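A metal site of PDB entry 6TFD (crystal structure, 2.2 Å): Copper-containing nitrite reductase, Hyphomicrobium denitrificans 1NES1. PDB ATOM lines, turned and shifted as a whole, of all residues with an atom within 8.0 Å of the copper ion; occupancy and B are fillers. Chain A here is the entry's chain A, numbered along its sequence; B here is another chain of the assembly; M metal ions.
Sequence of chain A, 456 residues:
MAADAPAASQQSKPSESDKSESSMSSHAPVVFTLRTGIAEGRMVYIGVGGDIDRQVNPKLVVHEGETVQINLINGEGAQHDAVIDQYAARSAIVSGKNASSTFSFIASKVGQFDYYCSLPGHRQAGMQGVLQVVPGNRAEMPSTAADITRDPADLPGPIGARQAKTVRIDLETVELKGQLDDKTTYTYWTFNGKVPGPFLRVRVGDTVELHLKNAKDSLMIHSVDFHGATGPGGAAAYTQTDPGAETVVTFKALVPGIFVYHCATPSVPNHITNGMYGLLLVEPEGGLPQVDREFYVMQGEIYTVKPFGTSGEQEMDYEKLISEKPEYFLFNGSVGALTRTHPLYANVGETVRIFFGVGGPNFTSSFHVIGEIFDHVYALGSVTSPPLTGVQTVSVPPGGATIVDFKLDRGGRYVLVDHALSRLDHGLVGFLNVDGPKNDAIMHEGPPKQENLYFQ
Gln 79 touches the copper ion.
Five residues have an atom within 4 Å of the copper ion: Gln 79, His 80, Cys 117, His 122 and Met 127.
A ring nitrogen (ND1) of His 80 binds the copper ion (2.0 Å).
A ring nitrogen (ND1) of His 122 binds the copper ion.
The side-chain sulfur (SG) of Cys 117 binds the copper ion.
SD of Met 127 is bound to the copper ion (2.6 Å).
The copper ion has four donor atoms within binding distance.
A ring nitrogen (NE2) of His 80 lies close to the side-chain hydroxyl of Thr 36 (3.4 Å).
The side-chain carboxylate (OE2) of Glu 76 is in hydrogen-bond range of a ring nitrogen (NE2) of His 80 (2.5 Å).
The backbone carbonyl oxygen (O) of His 80 sits at hydrogen-bond distance from the backbone NH (N) of Val 94, 2.8 Å away.
A ring nitrogen (ND1) of His 122 lies close to the backbone carbonyl oxygen of Gln 79.
The backbone NH of Leu 119 sits close to the side-chain sulfur of Cys 117, at 3.5 Å.
The backbone NH (N) of Asp 81 sits close to the side-chain sulfur (SG) of Cys 117 (3.6 Å).
The backbone NH (N) of Cys 117 lies within hydrogen-bond range of the side-chain hydroxyl (OH) of Tyr 45 (2.9 Å).
N of Met 127 lies within hydrogen-bond range of O of Met 43.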
ATOM      1  N   THR A  36      24.330  -4.696   3.273  1.00  0.00           N
ATOM      2  CA  THR A  36      24.219  -6.010   3.972  1.00  0.00           C
ATOM      3  C   THR A  36      22.946  -6.028   4.821  1.00  0.00           C
ATOM      4  O   THR A  36      22.562  -4.974   5.394  1.00  0.00           O
ATOM      5  CB  THR A  36      25.453  -6.310   4.823  1.00  0.00           C
ATOM      6  OG1 THR A  36      25.435  -5.424   5.946  1.00  0.00           O
ATOM      7  CG2 THR A  36      26.718  -6.176   4.024  1.00  0.00           C
ATOM      8  N   MET A  43      21.447 -14.151   5.838  1.00  0.00           N
ATOM      9  CA  MET A  43      22.309 -12.945   5.809  1.00  0.00           C
ATOM     10  C   MET A  43      22.861 -12.777   4.392  1.00  0.00           C
ATOM     11  O   MET A  43      23.570 -13.685   3.914  1.00  0.00           O
ATOM     12  CB  MET A  43      23.462 -13.079   6.799  1.00  0.00           C
ATOM     13  CG  MET A  43      24.131 -11.763   7.069  1.00  0.00           C
ATOM     14  SD  MET A  43      25.137 -11.853   8.562  1.00  0.00           S
ATOM     15  CE  MET A  43      26.191 -13.246   8.168  1.00  0.00           C
ATOM     16  N   VAL A  44      22.531 -11.662   3.751  1.00  0.00           N
ATOM     17  CA  VAL A  44      22.693 -11.441   2.286  1.00  0.00           C
ATOM     18  C   VAL A  44      23.204 -10.031   2.023  1.00  0.00           C
ATOM     19  O   VAL A  44      23.289  -9.201   2.938  1.00  0.00           O
ATOM     20  CB  VAL A  44      21.363 -11.678   1.571  1.00  0.00           C
ATOM     21  CG1 VAL A  44      20.908 -13.117   1.726  1.00  0.00           C
ATOM     22  CG2 VAL A  44      20.276 -10.714   2.021  1.00  0.00           C
ATOM     23  N   TYR A  45      23.563  -9.792   0.761  1.00  0.00           N
ATOM     24  CA  TYR A  45      23.750  -8.450   0.171  1.00  0.00           C
ATOM     25  C   TYR A  45      22.380  -8.063  -0.373  1.00  0.00           C
ATOM     26  O   TYR A  45      21.700  -8.984  -0.854  1.00  0.00           O
ATOM     27  CB  TYR A  45      24.814  -8.516  -0.922  1.00  0.00           C
ATOM     28  CG  TYR A  45      26.201  -8.912  -0.499  1.00  0.00           C
ATOM     29  CD1 TYR A  45      27.041  -8.001   0.097  1.00  0.00           C
ATOM     30  CD2 TYR A  45      26.702 -10.178  -0.755  1.00  0.00           C
ATOM     31  CE1 TYR A  45      28.348  -8.325   0.450  1.00  0.00           C
ATOM     32  CE2 TYR A  45      28.005 -10.524  -0.391  1.00  0.00           C
ATOM     33  CZ  TYR A  45      28.825  -9.592   0.202  1.00  0.00           C
ATOM     34  OH  TYR A  45      30.120  -9.877   0.566  1.00  0.00           O
ATOM     35  N   LEU A  72      30.017  -1.021  -0.935  1.00  0.00           N
ATOM     36  CA  LEU A  72      29.469  -1.822   0.198  1.00  0.00           C
ATOM     37  C   LEU A  72      29.072  -0.917   1.380  1.00  0.00           C
ATOM     38  O   LEU A  72      29.944  -0.209   1.916  1.00  0.00           O
ATOM     39  CB  LEU A  72      30.488  -2.862   0.654  1.00  0.00           C
ATOM     40  CG  LEU A  72      29.959  -3.832   1.709  1.00  0.00           C
ATOM     41  CD1 LEU A  72      28.813  -4.660   1.139  1.00  0.00           C
ATOM     42  CD2 LEU A  72      31.060  -4.737   2.218  1.00  0.00           C
ATOM     43  N   ASN A  74      27.326  -1.355   5.210  1.00  0.00           N
ATOM     44  CA  ASN A  74      26.920  -2.217   6.342  1.00  0.00           C
ATOM     45  C   ASN A  74      25.480  -1.844   6.742  1.00  0.00           C
ATOM     46  O   ASN A  74      25.252  -0.681   7.070  1.00  0.00           O
ATOM     47  CB  ASN A  74      27.882  -2.065   7.532  1.00  0.00           C
ATOM     48  CG  ASN A  74      27.587  -3.017   8.668  1.00  0.00           C
ATOM     49  OD1 ASN A  74      26.471  -3.044   9.186  1.00  0.00           O
ATOM     50  ND2 ASN A  74      28.586  -3.784   9.094  1.00  0.00           N
ATOM     51  N   GLU A  76      23.133  -3.972   8.965  1.00  0.00           N
ATOM     52  CA  GLU A  76      22.538  -4.548  10.210  1.00  0.00           C
ATOM     53  C   GLU A  76      23.538  -4.559  11.376  1.00  0.00           C
ATOM     54  O   GLU A  76      23.087  -4.666  12.515  1.00  0.00           O
ATOM     55  CB  GLU A  76      21.933  -5.932   9.925  1.00  0.00           C
ATOM     56  CG  GLU A  76      22.941  -7.073   9.836  1.00  0.00           C
ATOM     57  CD  GLU A  76      24.132  -6.857   8.922  1.00  0.00           C
ATOM     58  OE1 GLU A  76      23.955  -6.335   7.807  1.00  0.00           O
ATOM     59  OE2 GLU A  76      25.237  -7.189   9.339  1.00  0.00           O
ATOM     60  N   ALA A  78      26.807  -6.384  11.750  1.00  0.00           N
ATOM     61  CA  ALA A  78      27.866  -7.405  11.827  1.00  0.00           C
ATOM     62  C   ALA A  78      28.999  -6.972  10.886  1.00  0.00           C
ATOM     63  O   ALA A  78      28.769  -6.036  10.099  1.00  0.00           O
ATOM     64  CB  ALA A  78      27.290  -8.770  11.477  1.00  0.00           C
ATOM     65  N   GLN A  79      30.167  -7.612  10.976  1.00  0.00           N
ATOM     66  CA  GLN A  79      31.366  -7.297  10.160  1.00  0.00           C
ATOM     67  C   GLN A  79      31.199  -7.903   8.769  1.00  0.00           C
ATOM     68  O   GLN A  79      30.793  -9.042   8.679  1.00  0.00           O
ATOM     69  CB  GLN A  79      32.610  -7.802  10.871  1.00  0.00           C
ATOM     70  CG  GLN A  79      32.933  -7.006  12.119  1.00  0.00           C
ATOM     71  CD  GLN A  79      34.392  -7.161  12.498  1.00  0.00           C
ATOM     72  OE1 GLN A  79      34.870  -8.263  12.754  1.00  0.00           O
ATOM     73  NE2 GLN A  79      35.121  -6.051  12.478  1.00  0.00           N
ATOM     74  N   HIS A  80      31.475  -7.128   7.705  1.00  0.00           N
ATOM     75  CA  HIS A  80      31.348  -7.590   6.297  1.00  0.00           C
ATOM     76  C   HIS A  80      32.468  -7.047   5.393  1.00  0.00           C
ATOM     77  O   HIS A  80      32.997  -5.947   5.638  1.00  0.00           O
ATOM     78  CB  HIS A  80      30.001  -7.169   5.700  1.00  0.00           C
ATOM     79  CG  HIS A  80      28.836  -7.661   6.492  1.00  0.00           C
ATOM     80  ND1 HIS A  80      28.633  -8.994   6.741  1.00  0.00           N
ATOM     81  CD2 HIS A  80      27.830  -7.004   7.087  1.00  0.00           C
ATOM     82  CE1 HIS A  80      27.536  -9.137   7.446  1.00  0.00           C
ATOM     83  NE2 HIS A  80      27.024  -7.925   7.680  1.00  0.00           N
ATOM     84  N   ASP A  81      32.773  -7.805   4.353  1.00  0.00           N
ATOM     85  CA  ASP A  81      33.484  -7.309   3.155  1.00  0.00           C
ATOM     86  C   ASP A  81      32.808  -7.920   1.929  1.00  0.00           C
ATOM     87  O   ASP A  81      31.742  -8.557   2.083  1.00  0.00           O
ATOM     88  CB  ASP A  81      34.987  -7.573   3.280  1.00  0.00           C
ATOM     89  CG  ASP A  81      35.379  -9.036   3.291  1.00  0.00           C
ATOM     90  OD1 ASP A  81      34.497  -9.892   3.059  1.00  0.00           O
ATOM     91  OD2 ASP A  81      36.563  -9.321   3.490  1.00  0.00           O
ATOM     92  N   ALA A  82      33.359  -7.653   0.748  1.00  0.00           N
ATOM     93  CA  ALA A  82      32.955  -8.239  -0.547  1.00  0.00           C
ATOM     94  C   ALA A  82      34.241  -8.532  -1.316  1.00  0.00           C
ATOM     95  O   ALA A  82      35.126  -7.640  -1.364  1.00  0.00           O
ATOM     96  CB  ALA A  82      32.052  -7.303  -1.297  1.00  0.00           C
ATOM     97  N   VAL A  94      33.782  -3.586   6.882  1.00  0.00           N
ATOM     98  CA  VAL A  94      32.870  -2.556   7.459  1.00  0.00           C
ATOM     99  C   VAL A  94      32.186  -3.159   8.693  1.00  0.00           C
ATOM    100  O   VAL A  94      31.631  -4.264   8.602  1.00  0.00           O
ATOM    101  CB  VAL A  94      31.891  -2.008   6.402  1.00  0.00           C
ATOM    102  CG1 VAL A  94      32.643  -1.240   5.331  1.00  0.00           C
ATOM    103  CG2 VAL A  94      31.019  -3.084   5.765  1.00  0.00           C
ATOM    104  N   TYR A 116      31.489 -12.311  -2.593  1.00  0.00           N
ATOM    105  CA  TYR A 116      31.197 -13.017  -1.331  1.00  0.00           C
ATOM    106  C   TYR A 116      31.865 -12.311  -0.150  1.00  0.00           C
ATOM    107  O   TYR A 116      32.881 -11.619  -0.351  1.00  0.00           O
ATOM    108  CB  TYR A 116      31.622 -14.494  -1.443  1.00  0.00           C
ATOM    109  CG  TYR A 116      33.110 -14.717  -1.419  1.00  0.00           C
ATOM    110  CD1 TYR A 116      33.811 -14.845  -0.231  1.00  0.00           C
ATOM    111  CD2 TYR A 116      33.822 -14.789  -2.601  1.00  0.00           C
ATOM    112  CE1 TYR A 116      35.183 -15.034  -0.226  1.00  0.00           C
ATOM    113  CE2 TYR A 116      35.187 -14.967  -2.614  1.00  0.00           C
ATOM    114  CZ  TYR A 116      35.871 -15.091  -1.423  1.00  0.00           C
ATOM    115  OH  TYR A 116      37.230 -15.250  -1.466  1.00  0.00           O
ATOM    116  N   CYS A 117      31.316 -12.527   1.033  1.00  0.00           N
ATOM    117  CA  CYS A 117      31.848 -12.006   2.325  1.00  0.00           C
ATOM    118  C   CYS A 117      32.786 -13.065   2.924  1.00  0.00           C
ATOM    119  O   CYS A 117      32.356 -14.216   3.070  1.00  0.00           O
ATOM    120  CB  CYS A 117      30.739 -11.653   3.302  1.00  0.00           C
ATOM    121  SG  CYS A 117      31.399 -11.118   4.892  1.00  0.00           S
ATOM    122  N   SER A 118      34.014 -12.668   3.276  1.00  0.00           N
ATOM    123  CA  SER A 118      35.109 -13.541   3.774  1.00  0.00           C
ATOM    124  C   SER A 118      35.095 -13.669   5.314  1.00  0.00           C
ATOM    125  O   SER A 118      35.951 -14.413   5.845  1.00  0.00           O
ATOM    126  CB  SER A 118      36.437 -13.026   3.320  1.00  0.00           C
ATOM    127  OG  SER A 118      36.853 -11.941   4.131  1.00  0.00           O
ATOM    128  N   LEU A 119      34.193 -12.968   6.010  1.00  0.00           N
ATOM    129  CA  LEU A 119      34.111 -13.080   7.492  1.00  0.00           C
ATOM    130  C   LEU A 119      33.668 -14.502   7.843  1.00  0.00           C
ATOM    131  O   LEU A 119      32.813 -15.078   7.151  1.00  0.00           O
ATOM    132  CB  LEU A 119      33.162 -12.025   8.069  1.00  0.00           C
ATOM    133  CG  LEU A 119      33.785 -10.682   8.437  1.00  0.00           C
ATOM    134  CD1 LEU A 119      34.878 -10.843   9.504  1.00  0.00           C
ATOM    135  CD2 LEU A 119      34.331  -9.975   7.201  1.00  0.00           C
ATOM    136  N   PRO A 120      34.195 -15.104   8.933  1.00  0.00           N
ATOM    137  CA  PRO A 120      33.838 -16.471   9.307  1.00  0.00           C
ATOM    138  C   PRO A 120      32.321 -16.731   9.256  1.00  0.00           C
ATOM    139  O   PRO A 120      31.551 -16.001   9.875  1.00  0.00           O
ATOM    140  CB  PRO A 120      34.368 -16.601  10.746  1.00  0.00           C
ATOM    141  CG  PRO A 120      35.462 -15.567  10.863  1.00  0.00           C
ATOM    142  CD  PRO A 120      35.067 -14.454   9.924  1.00  0.00           C
ATOM    143  N   GLY A 121      31.908 -17.747   8.495  1.00  0.00           N
ATOM    144  CA  GLY A 121      30.528 -18.226   8.407  1.00  0.00           C
ATOM    145  C   GLY A 121      29.672 -17.487   7.383  1.00  0.00           C
ATOM    146  O   GLY A 121      28.686 -18.073   6.902  1.00  0.00           O
ATOM    147  N   HIS A 122      30.011 -16.230   7.061  1.00  0.00           N
ATOM    148  CA  HIS A 122      29.077 -15.298   6.370  1.00  0.00           C
ATOM    149  C   HIS A 122      28.752 -15.839   4.984  1.00  0.00           C
ATOM    150  O   HIS A 122      27.601 -15.707   4.569  1.00  0.00           O
ATOM    151  CB  HIS A 122      29.629 -13.870   6.390  1.00  0.00           C
ATOM    152  CG  HIS A 122      29.503 -13.207   7.727  1.00  0.00           C
ATOM    153  ND1 HIS A 122      29.387 -11.841   7.887  1.00  0.00           N
ATOM    154  CD2 HIS A 122      29.476 -13.720   8.971  1.00  0.00           C
ATOM    155  CE1 HIS A 122      29.261 -11.549   9.165  1.00  0.00           C
ATOM    156  NE2 HIS A 122      29.329 -12.684   9.854  1.00  0.00           N
ATOM    157  N   ARG A 123      29.703 -16.481   4.304  1.00  0.00           N
ATOM    158  CA  ARG A 123      29.452 -16.999   2.925  1.00  0.00           C
ATOM    159  C   ARG A 123      28.426 -18.141   2.993  1.00  0.00           C
ATOM    160  O   ARG A 123      27.398 -18.100   2.268  1.00  0.00           O
ATOM    161  CB  ARG A 123      30.760 -17.464   2.278  1.00  0.00           C
ATOM    162  CG  ARG A 123      30.643 -17.760   0.788  1.00  0.00           C
ATOM    163  CD  ARG A 123      31.983 -18.147   0.178  1.00  0.00           C
ATOM    164  NE  ARG A 123      31.850 -18.140  -1.274  1.00  0.00           N
ATOM    165  CZ  ARG A 123      32.842 -18.117  -2.136  1.00  0.00           C
ATOM    166  NH1 ARG A 123      32.590 -18.067  -3.443  1.00  0.00           N
ATOM    167  NH2 ARG A 123      34.091 -18.114  -1.711  1.00  0.00           N
ATOM    168  N   ALA A 125      26.330 -18.601   5.386  1.00  0.00           N
ATOM    169  CA  ALA A 125      25.066 -17.975   5.888  1.00  0.00           C
ATOM    170  C   ALA A 125      24.278 -17.262   4.776  1.00  0.00           C
ATOM    171  O   ALA A 125      23.104 -16.932   5.073  1.00  0.00           O
ATOM    172  CB  ALA A 125      25.380 -17.027   7.011  1.00  0.00           C
ATOM    173  N   MET A 127      25.819 -14.747   2.164  1.00  0.00           N
ATOM    174  CA  MET A 127      26.484 -13.571   1.538  1.00  0.00           C
ATOM    175  C   MET A 127      27.313 -14.064   0.338  1.00  0.00           C
ATOM    176  O   MET A 127      28.542 -14.275   0.476  1.00  0.00           O
ATOM    177  CB  MET A 127      27.350 -12.826   2.554  1.00  0.00           C
ATOM    178  CG  MET A 127      26.549 -12.422   3.767  1.00  0.00           C
ATOM    179  SD  MET A 127      27.362 -11.185   4.792  1.00  0.00           S
ATOM    180  CE  MET A 127      26.755  -9.733   3.934  1.00  0.00           C
ATOM    181  N   ALA B 125      30.068 -17.347  13.028  1.00  0.00           N
ATOM    182  CA  ALA B 125      29.624 -15.936  12.936  1.00  0.00           C
ATOM    183  C   ALA B 125      29.239 -15.359  14.307  1.00  0.00           C
ATOM    184  O   ALA B 125      28.880 -14.165  14.327  1.00  0.00           O
ATOM    185  CB  ALA B 125      28.488 -15.815  11.954  1.00  0.00           C
HETATM  186 CU    CU M   1      29.529 -10.631   6.083  1.00  0.00          CU
